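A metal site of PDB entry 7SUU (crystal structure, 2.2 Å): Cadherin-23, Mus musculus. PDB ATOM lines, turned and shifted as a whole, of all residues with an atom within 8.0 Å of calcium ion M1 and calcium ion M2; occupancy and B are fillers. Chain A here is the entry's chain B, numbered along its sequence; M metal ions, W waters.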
ATOM      1  N   SER A   3       5.399 -13.473  29.476  1.00  0.00           N
ATOM      2  CA  SER A   3       4.525 -14.266  28.502  1.00  0.00           C
ATOM      3  C   SER A   3       3.454 -13.415  27.751  1.00  0.00           C
ATOM      4  O   SER A   3       3.197 -13.756  26.579  1.00  0.00           O
ATOM      5  CB  SER A   3       3.912 -15.467  29.163  1.00  0.00           C
ATOM      6  OG  SER A   3       4.176 -16.645  28.393  1.00  0.00           O
ATOM      7  N   ASP A   4       2.836 -12.381  28.333  1.00  0.00           N
ATOM      8  CA  ASP A   4       1.759 -11.575  27.667  1.00  0.00           C
ATOM      9  C   ASP A   4       2.308 -10.812  26.446  1.00  0.00           C
ATOM     10  O   ASP A   4       3.360 -10.192  26.545  1.00  0.00           O
ATOM     11  CB  ASP A   4       1.063 -10.580  28.619  1.00  0.00           C
ATOM     12  CG  ASP A   4       0.001  -9.690  27.958  1.00  0.00           C
ATOM     13  OD1 ASP A   4      -1.003 -10.229  27.395  1.00  0.00           O
ATOM     14  OD2 ASP A   4       0.191  -8.453  27.980  1.00  0.00           O
ATOM     15  N   VAL A   5       1.629 -10.904  25.302  1.00  0.00           N
ATOM     16  CA  VAL A   5       1.874 -10.024  24.142  1.00  0.00           C
ATOM     17  C   VAL A   5       0.639  -9.151  23.968  1.00  0.00           C
ATOM     18  O   VAL A   5      -0.434  -9.360  24.588  1.00  0.00           O
ATOM     19  CB  VAL A   5       2.205 -10.794  22.848  1.00  0.00           C
ATOM     20  CG1 VAL A   5       3.257 -11.887  23.048  1.00  0.00           C
ATOM     21  CG2 VAL A   5       0.985 -11.370  22.183  1.00  0.00           C
ATOM     22  N   ASN A   6       0.821  -8.161  23.120  1.00  0.00           N
ATOM     23  CA  ASN A   6      -0.218  -7.174  22.788  1.00  0.00           C
ATOM     24  C   ASN A   6      -1.083  -7.820  21.732  1.00  0.00           C
ATOM     25  O   ASN A   6      -0.680  -7.830  20.552  1.00  0.00           O
ATOM     26  CB  ASN A   6       0.377  -5.859  22.309  1.00  0.00           C
ATOM     27  CG  ASN A   6      -0.660  -4.776  22.457  1.00  0.00           C
ATOM     28  OD1 ASN A   6      -1.585  -4.927  23.251  1.00  0.00           O
ATOM     29  ND2 ASN A   6      -0.493  -3.708  21.699  1.00  0.00           N
ATOM     30  N   ASP A   7      -2.215  -8.381  22.161  1.00  0.00           N
ATOM     31  CA  ASP A   7      -3.149  -8.994  21.205  1.00  0.00           C
ATOM     32  C   ASP A   7      -4.551  -8.516  21.522  1.00  0.00           C
ATOM     33  O   ASP A   7      -5.451  -9.193  21.124  1.00  0.00           O
ATOM     34  CB  ASP A   7      -2.961 -10.496  21.199  1.00  0.00           C
ATOM     35  CG  ASP A   7      -3.311 -11.192  22.502  1.00  0.00           C
ATOM     36  OD1 ASP A   7      -3.185 -10.565  23.591  1.00  0.00           O
ATOM     37  OD2 ASP A   7      -3.708 -12.352  22.402  1.00  0.00           O
ATOM     38  N   ASN A   8      -4.702  -7.393  22.242  1.00  0.00           N
ATOM     39  CA  ASN A   8      -6.014  -6.801  22.610  1.00  0.00           C
ATOM     40  C   ASN A   8      -5.978  -5.313  22.372  1.00  0.00           C
ATOM     41  O   ASN A   8      -5.009  -4.632  22.840  1.00  0.00           O
ATOM     42  CB  ASN A   8      -6.409  -7.069  24.060  1.00  0.00           C
ATOM     43  CG  ASN A   8      -6.826  -8.514  24.233  1.00  0.00           C
ATOM     44  OD1 ASN A   8      -8.009  -8.805  24.104  1.00  0.00           O
ATOM     45  ND2 ASN A   8      -5.874  -9.404  24.508  1.00  0.00           N
ATOM     46  N   ARG A   9      -6.974  -4.861  21.630  1.00  0.00           N
ATOM     47  CA  ARG A   9      -7.257  -3.421  21.358  1.00  0.00           C
ATOM     48  C   ARG A   9      -8.002  -2.881  22.572  1.00  0.00           C
ATOM     49  O   ARG A   9      -8.715  -3.644  23.252  1.00  0.00           O
ATOM     50  CB  ARG A   9      -7.966  -3.307  20.002  1.00  0.00           C
ATOM     51  CG  ARG A   9      -9.410  -3.788  19.943  1.00  0.00           C
ATOM     52  CD  ARG A   9     -10.039  -3.262  18.663  1.00  0.00           C
ATOM     53  NE  ARG A   9     -11.409  -3.674  18.558  1.00  0.00           N
ATOM     54  CZ  ARG A   9     -12.454  -3.122  19.190  1.00  0.00           C
ATOM     55  NH1 ARG A   9     -13.668  -3.642  19.012  1.00  0.00           N
ATOM     56  NH2 ARG A   9     -12.326  -2.066  19.987  1.00  0.00           N
ATOM     57  N   PRO A  10      -7.778  -1.589  22.923  1.00  0.00           N
ATOM     58  CA  PRO A  10      -8.637  -0.897  23.873  1.00  0.00           C
ATOM     59  C   PRO A  10     -10.098  -0.933  23.386  1.00  0.00           C
ATOM     60  O   PRO A  10     -10.339  -0.890  22.186  1.00  0.00           O
ATOM     61  CB  PRO A  10      -8.119   0.537  23.877  1.00  0.00           C
ATOM     62  CG  PRO A  10      -6.678   0.392  23.445  1.00  0.00           C
ATOM     63  CD  PRO A  10      -6.699  -0.731  22.435  1.00  0.00           C
ATOM     64  N   THR A  39     -11.037   0.250  28.188  1.00  0.00           N
ATOM     65  CA  THR A  39     -10.356  -0.857  28.886  1.00  0.00           C
ATOM     66  C   THR A  39      -9.475  -1.620  27.882  1.00  0.00           C
ATOM     67  O   THR A  39      -9.846  -1.667  26.688  1.00  0.00           O
ATOM     68  CB  THR A  39     -11.394  -1.818  29.501  1.00  0.00           C
ATOM     69  OG1 THR A  39     -12.319  -2.149  28.463  1.00  0.00           O
ATOM     70  CG2 THR A  39     -12.126  -1.222  30.678  1.00  0.00           C
ATOM     71  N   ASP A  40      -8.415  -2.285  28.384  1.00  0.00           N
ATOM     72  CA  ASP A  40      -7.493  -3.130  27.589  1.00  0.00           C
ATOM     73  C   ASP A  40      -7.168  -4.376  28.440  1.00  0.00           C
ATOM     74  O   ASP A  40      -6.718  -4.219  29.601  1.00  0.00           O
ATOM     75  CB  ASP A  40      -6.258  -2.325  27.136  1.00  0.00           C
ATOM     76  CG  ASP A  40      -5.383  -2.944  26.051  1.00  0.00           C
ATOM     77  OD1 ASP A  40      -5.039  -4.149  26.171  1.00  0.00           O
ATOM     78  OD2 ASP A  40      -5.009  -2.204  25.113  1.00  0.00           O
ATOM     79  N   ASN A  41      -7.374  -5.564  27.866  1.00  0.00           N
ATOM     80  CA  ASN A  41      -7.358  -6.860  28.593  1.00  0.00           C
ATOM     81  C   ASN A  41      -5.938  -7.443  28.607  1.00  0.00           C
ATOM     82  O   ASN A  41      -5.786  -8.520  29.148  1.00  0.00           O
ATOM     83  CB  ASN A  41      -8.323  -7.867  27.981  1.00  0.00           C
ATOM     84  CG  ASN A  41      -9.764  -7.442  28.165  1.00  0.00           C
ATOM     85  OD1 ASN A  41     -10.063  -6.522  28.929  1.00  0.00           O
ATOM     86  ND2 ASN A  41     -10.662  -8.082  27.448  1.00  0.00           N
ATOM     87  N   ASP A  42      -4.951  -6.754  28.045  1.00  0.00           N
ATOM     88  CA  ASP A  42      -3.521  -7.126  28.159  1.00  0.00           C
ATOM     89  C   ASP A  42      -2.985  -6.690  29.533  1.00  0.00           C
ATOM     90  O   ASP A  42      -3.729  -6.035  30.260  1.00  0.00           O
ATOM     91  CB  ASP A  42      -2.713  -6.561  26.983  1.00  0.00           C
ATOM     92  CG  ASP A  42      -3.135  -7.168  25.658  1.00  0.00           C
ATOM     93  OD1 ASP A  42      -3.151  -8.414  25.573  1.00  0.00           O
ATOM     94  OD2 ASP A  42      -3.501  -6.393  24.748  1.00  0.00           O
ATOM     95  N   GLU A  43      -1.742  -7.057  29.873  1.00  0.00           N
ATOM     96  CA  GLU A  43      -1.033  -6.665  31.128  1.00  0.00           C
ATOM     97  C   GLU A  43      -0.013  -5.565  30.838  1.00  0.00           C
ATOM     98  O   GLU A  43       0.454  -5.448  29.679  1.00  0.00           O
ATOM     99  CB  GLU A  43      -0.276  -7.852  31.740  1.00  0.00           C
ATOM    100  CG  GLU A  43      -1.042  -8.606  32.810  1.00  0.00           C
ATOM    101  CD  GLU A  43      -1.662  -9.918  32.357  1.00  0.00           C
ATOM    102  OE1 GLU A  43      -1.283 -10.428  31.283  1.00  0.00           O
ATOM    103  OE2 GLU A  43      -2.535 -10.448  33.090  1.00  0.00           O
ATOM    104  N   GLY A  44       0.416  -4.847  31.883  1.00  0.00           N
ATOM    105  CA  GLY A  44       1.508  -3.856  31.822  1.00  0.00           C
ATOM    106  C   GLY A  44       1.284  -2.859  30.701  1.00  0.00           C
ATOM    107  O   GLY A  44       0.125  -2.483  30.461  1.00  0.00           O
ATOM    108  N   LEU A  45       2.356  -2.459  30.028  1.00  0.00           N
ATOM    109  CA  LEU A  45       2.349  -1.475  28.915  1.00  0.00           C
ATOM    110  C   LEU A  45       1.369  -1.891  27.817  1.00  0.00           C
ATOM    111  O   LEU A  45       0.661  -1.007  27.305  1.00  0.00           O
ATOM    112  CB  LEU A  45       3.770  -1.347  28.374  1.00  0.00           C
ATOM    113  CG  LEU A  45       4.735  -0.538  29.240  1.00  0.00           C
ATOM    114  CD1 LEU A  45       6.054  -0.336  28.512  1.00  0.00           C
ATOM    115  CD2 LEU A  45       4.109   0.797  29.634  1.00  0.00           C
ATOM    116  N   ASN A  46       1.268  -3.187  27.534  1.00  0.00           N
ATOM    117  CA  ASN A  46       0.321  -3.735  26.528  1.00  0.00           C
ATOM    118  C   ASN A  46      -1.122  -3.341  26.914  1.00  0.00           C
ATOM    119  O   ASN A  46      -1.991  -3.349  26.025  1.00  0.00           O
ATOM    120  CB  ASN A  46       0.458  -5.246  26.371  1.00  0.00           C
ATOM    121  CG  ASN A  46       1.800  -5.704  25.846  1.00  0.00           C
ATOM    122  OD1 ASN A  46       2.533  -4.959  25.188  1.00  0.00           O
ATOM    123  ND2 ASN A  46       2.118  -6.977  26.090  1.00  0.00           N
ATOM    124  N   GLY A  47      -1.379  -3.163  28.210  1.00  0.00           N
ATOM    125  CA  GLY A  47      -2.723  -2.909  28.786  1.00  0.00           C
ATOM    126  C   GLY A  47      -2.939  -1.460  29.199  1.00  0.00           C
ATOM    127  O   GLY A  47      -3.994  -1.135  29.776  1.00  0.00           O
ATOM    128  N   ALA A  48      -1.968  -0.610  28.961  1.00  0.00           N
ATOM    129  CA  ALA A  48      -1.961   0.788  29.450  1.00  0.00           C
ATOM    130  C   ALA A  48      -2.638   1.655  28.383  1.00  0.00           C
ATOM    131  O   ALA A  48      -2.136   1.695  27.256  1.00  0.00           O
ATOM    132  CB  ALA A  48      -0.541   1.236  29.718  1.00  0.00           C
ATOM    133  N   VAL A  49      -3.737   2.322  28.730  1.00  0.00           N
ATOM    134  CA  VAL A  49      -4.548   3.110  27.780  1.00  0.00           C
ATOM    135  C   VAL A  49      -4.172   4.597  27.847  1.00  0.00           C
ATOM    136  O   VAL A  49      -4.075   5.174  28.971  1.00  0.00           O
ATOM    137  CB  VAL A  49      -6.036   2.867  28.036  1.00  0.00           C
ATOM    138  CG1 VAL A  49      -6.887   3.698  27.081  1.00  0.00           C
ATOM    139  CG2 VAL A  49      -6.364   1.378  27.903  1.00  0.00           C
ATOM    140  N   SER A  95      -5.416   4.201  22.641  1.00  0.00           N
ATOM    141  CA  SER A  95      -4.204   3.426  22.250  1.00  0.00           C
ATOM    142  C   SER A  95      -3.650   2.759  23.484  1.00  0.00           C
ATOM    143  O   SER A  95      -3.772   3.325  24.571  1.00  0.00           O
ATOM    144  CB  SER A  95      -3.132   4.324  21.677  1.00  0.00           C
ATOM    145  OG  SER A  95      -3.658   5.158  20.668  1.00  0.00           O
ATOM    146  N   ASP A  96      -2.997   1.628  23.322  1.00  0.00           N
ATOM    147  CA  ASP A  96      -2.159   1.074  24.417  1.00  0.00           C
ATOM    148  C   ASP A  96      -0.705   1.502  24.147  1.00  0.00           C
ATOM    149  O   ASP A  96      -0.451   2.146  23.112  1.00  0.00           O
ATOM    150  CB  ASP A  96      -2.435  -0.418  24.539  1.00  0.00           C
ATOM    151  CG  ASP A  96      -2.087  -1.209  23.293  1.00  0.00           C
ATOM    152  OD1 ASP A  96      -1.182  -0.823  22.595  1.00  0.00           O
ATOM    153  OD2 ASP A  96      -2.735  -2.199  23.046  1.00  0.00           O
ATOM    154  N   LEU A  97       0.207   1.213  25.072  1.00  0.00           N
ATOM    155  CA  LEU A  97       1.666   1.448  24.901  1.00  0.00           C
ATOM    156  C   LEU A  97       2.377   0.117  24.594  1.00  0.00           C
ATOM    157  O   LEU A  97       3.525  -0.064  25.015  1.00  0.00           O
ATOM    158  CB  LEU A  97       2.177   2.102  26.196  1.00  0.00           C
ATOM    159  CG  LEU A  97       1.631   3.514  26.449  1.00  0.00           C
ATOM    160  CD1 LEU A  97       1.939   3.966  27.860  1.00  0.00           C
ATOM    161  CD2 LEU A  97       2.173   4.511  25.394  1.00  0.00           C
ATOM    162  N   GLY A  98       1.728  -0.755  23.844  1.00  0.00           N
ATOM    163  CA  GLY A  98       2.171  -2.152  23.671  1.00  0.00           C
ATOM    164  C   GLY A  98       3.470  -2.279  22.891  1.00  0.00           C
ATOM    165  O   GLY A  98       3.697  -1.443  21.991  1.00  0.00           O
ATOM    166  N   GLN A  99       4.335  -3.146  23.418  1.00  0.00           N
ATOM    167  CA  GLN A  99       5.154  -4.184  22.741  1.00  0.00           C
ATOM    168  C   GLN A  99       5.974  -3.600  21.603  1.00  0.00           C
ATOM    169  O   GLN A  99       6.464  -2.475  21.743  1.00  0.00           O
ATOM    170  CB  GLN A  99       4.235  -5.308  22.276  1.00  0.00           C
ATOM    171  CG  GLN A  99       4.558  -6.655  22.908  1.00  0.00           C
ATOM    172  CD  GLN A  99       4.096  -7.819  22.053  1.00  0.00           C
ATOM    173  OE1 GLN A  99       3.085  -7.745  21.354  1.00  0.00           O
ATOM    174  NE2 GLN A  99       4.854  -8.915  22.096  1.00  0.00           N
ATOM    175  N   VAL A 101       4.321  -3.312  18.627  1.00  0.00           N
ATOM    176  CA  VAL A 101       3.214  -2.558  17.965  1.00  0.00           C
ATOM    177  C   VAL A 101       2.098  -2.216  18.951  1.00  0.00           C
ATOM    178  O   VAL A 101       1.386  -3.111  19.417  1.00  0.00           O
ATOM    179  CB  VAL A 101       2.615  -3.325  16.780  1.00  0.00           C
ATOM    180  CG1 VAL A 101       1.773  -2.396  15.924  1.00  0.00           C
ATOM    181  CG2 VAL A 101       3.687  -4.024  15.964  1.00  0.00           C
ATOM    182  N   PRO A 102       1.798  -0.917  19.138  1.00  0.00           N
ATOM    183  CA  PRO A 102       0.570  -0.521  19.815  1.00  0.00           C
ATOM    184  C   PRO A 102      -0.697  -0.863  19.017  1.00  0.00           C
ATOM    185  O   PRO A 102      -0.678  -0.901  17.792  1.00  0.00           O
ATOM    186  CB  PRO A 102       0.687   1.017  19.942  1.00  0.00           C
ATOM    187  CG  PRO A 102       2.138   1.341  19.667  1.00  0.00           C
ATOM    188  CD  PRO A 102       2.561   0.262  18.675  1.00  0.00           C
ATOM    189  N   TYR A 103      -1.796  -1.093  19.743  1.00  0.00           N
ATOM    190  CA  TYR A 103      -3.171  -1.190  19.208  1.00  0.00           C
ATOM    191  C   TYR A 103      -3.864   0.153  19.505  1.00  0.00           C
ATOM    192  O   TYR A 103      -3.591   0.742  20.563  1.00  0.00           O
ATOM    193  CB  TYR A 103      -3.870  -2.417  19.784  1.00  0.00           C
ATOM    194  CG  TYR A 103      -3.451  -3.752  19.205  1.00  0.00           C
ATOM    195  CD1 TYR A 103      -2.137  -4.180  19.237  1.00  0.00           C
ATOM    196  CD2 TYR A 103      -4.381  -4.606  18.641  1.00  0.00           C
ATOM    197  CE1 TYR A 103      -1.752  -5.402  18.712  1.00  0.00           C
ATOM    198  CE2 TYR A 103      -4.023  -5.836  18.117  1.00  0.00           C
ATOM    199  CZ  TYR A 103      -2.698  -6.246  18.157  1.00  0.00           C
ATOM    200  OH  TYR A 103      -2.344  -7.456  17.656  1.00  0.00           O
ATOM    201  N   GLU A 104      -4.694   0.629  18.570  1.00  0.00           N
ATOM    202  CA  GLU A 104      -5.482   1.879  18.708  1.00  0.00           C
ATOM    203  C   GLU A 104      -6.928   1.557  18.328  1.00  0.00           C
ATOM    204  O   GLU A 104      -7.109   0.737  17.434  1.00  0.00           O
ATOM    205  CB  GLU A 104      -4.973   3.008  17.805  1.00  0.00           C
ATOM    206  CG  GLU A 104      -3.462   3.266  17.902  1.00  0.00           C
ATOM    207  CD  GLU A 104      -2.936   4.566  17.297  1.00  0.00           C
ATOM    208  OE1 GLU A 104      -3.700   5.540  17.233  1.00  0.00           O
ATOM    209  OE2 GLU A 104      -1.753   4.606  16.924  1.00  0.00           O
HETATM  210 CA    CA M   1      -2.143 -10.491  25.612  1.00  0.00          CA
HETATM  211 CA    CA M   2      -3.483  -4.038  24.319  1.00  0.00          CA
HETATM  212  O   HOH W   1      -4.022 -11.595  26.602  1.00  0.00           O
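OD2 of Asp 4 sits at hydrogen-bond distance from ND2 of Asn 46. OD2 of Asp 4 lies within hydrogen-bond range of N of Glu 43 (3.0 Å). The side-chain amide nitrogen (ND2) of Asn 8 lies close to the side-chain carboxylate (OD1) of Asp 7, at 3.1 Å. O of Asn 6 sits close to OH of Tyr 103, at 3.4 Å. ND2 of Asn 6 is in hydrogen-bond range of O of Val 101 (3.0 Å). The backbone NH (N) of Asn 6 is in hydrogen-bond range of the side-chain amide oxygen (OE1) of Gln 99 (2.9 Å). The side-chain carboxylate of Asp 96 sits at hydrogen-bond distance from the backbone NH of Tyr 103 (2.9 Å). N of Gln 99 sits at hydrogen-bond distance from OD1 of Asn 46, at 3.1 Å.
Along chain A the residues within 4 Å of calcium ion M1 span positions 4 to 42.
Within 4 Å of calcium ion M2: Asn 6, Asn 8, Asp 40, Asp 42, Asn 46 and Asp 96. The nearest printed residue that does not touch calcium ion M2 is Arg 9 (4.5 Å).
Calcium ion M1 is bound by the side-chain carboxylate of Asp 4 (2.1 Å), the side-chain carboxylate of Asp 7 (2.3 Å), the backbone carbonyl oxygen of Val 5 (2.3 Å), the side-chain carboxylate of Asp 42 (2.3 Å) and water W1 (2.4 Å). Calcium ion M1 has five donor atoms within binding distance.
Calcium ion M2 is bound by the backbone carbonyl oxygen (O) of Asn 8 (2.2 Å), the side-chain amide oxygen (OD1) of Asn 6 (2.4 Å), the side-chain carboxylate (OD2) of Asp 96 (2.4 Å), the backbone carbonyl oxygen (O) of Asn 46 (2.4 Å), the side-chain carboxylate (OD2) of Asp 42 (2.4 Å), the side-chain carboxylate (OD1) of Asp 40 (2.4 Å) and the side-chain carboxylate (OD2) of Asp 40 (2.5 Å). Calcium ion M2 has seven donor atoms within binding distance.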
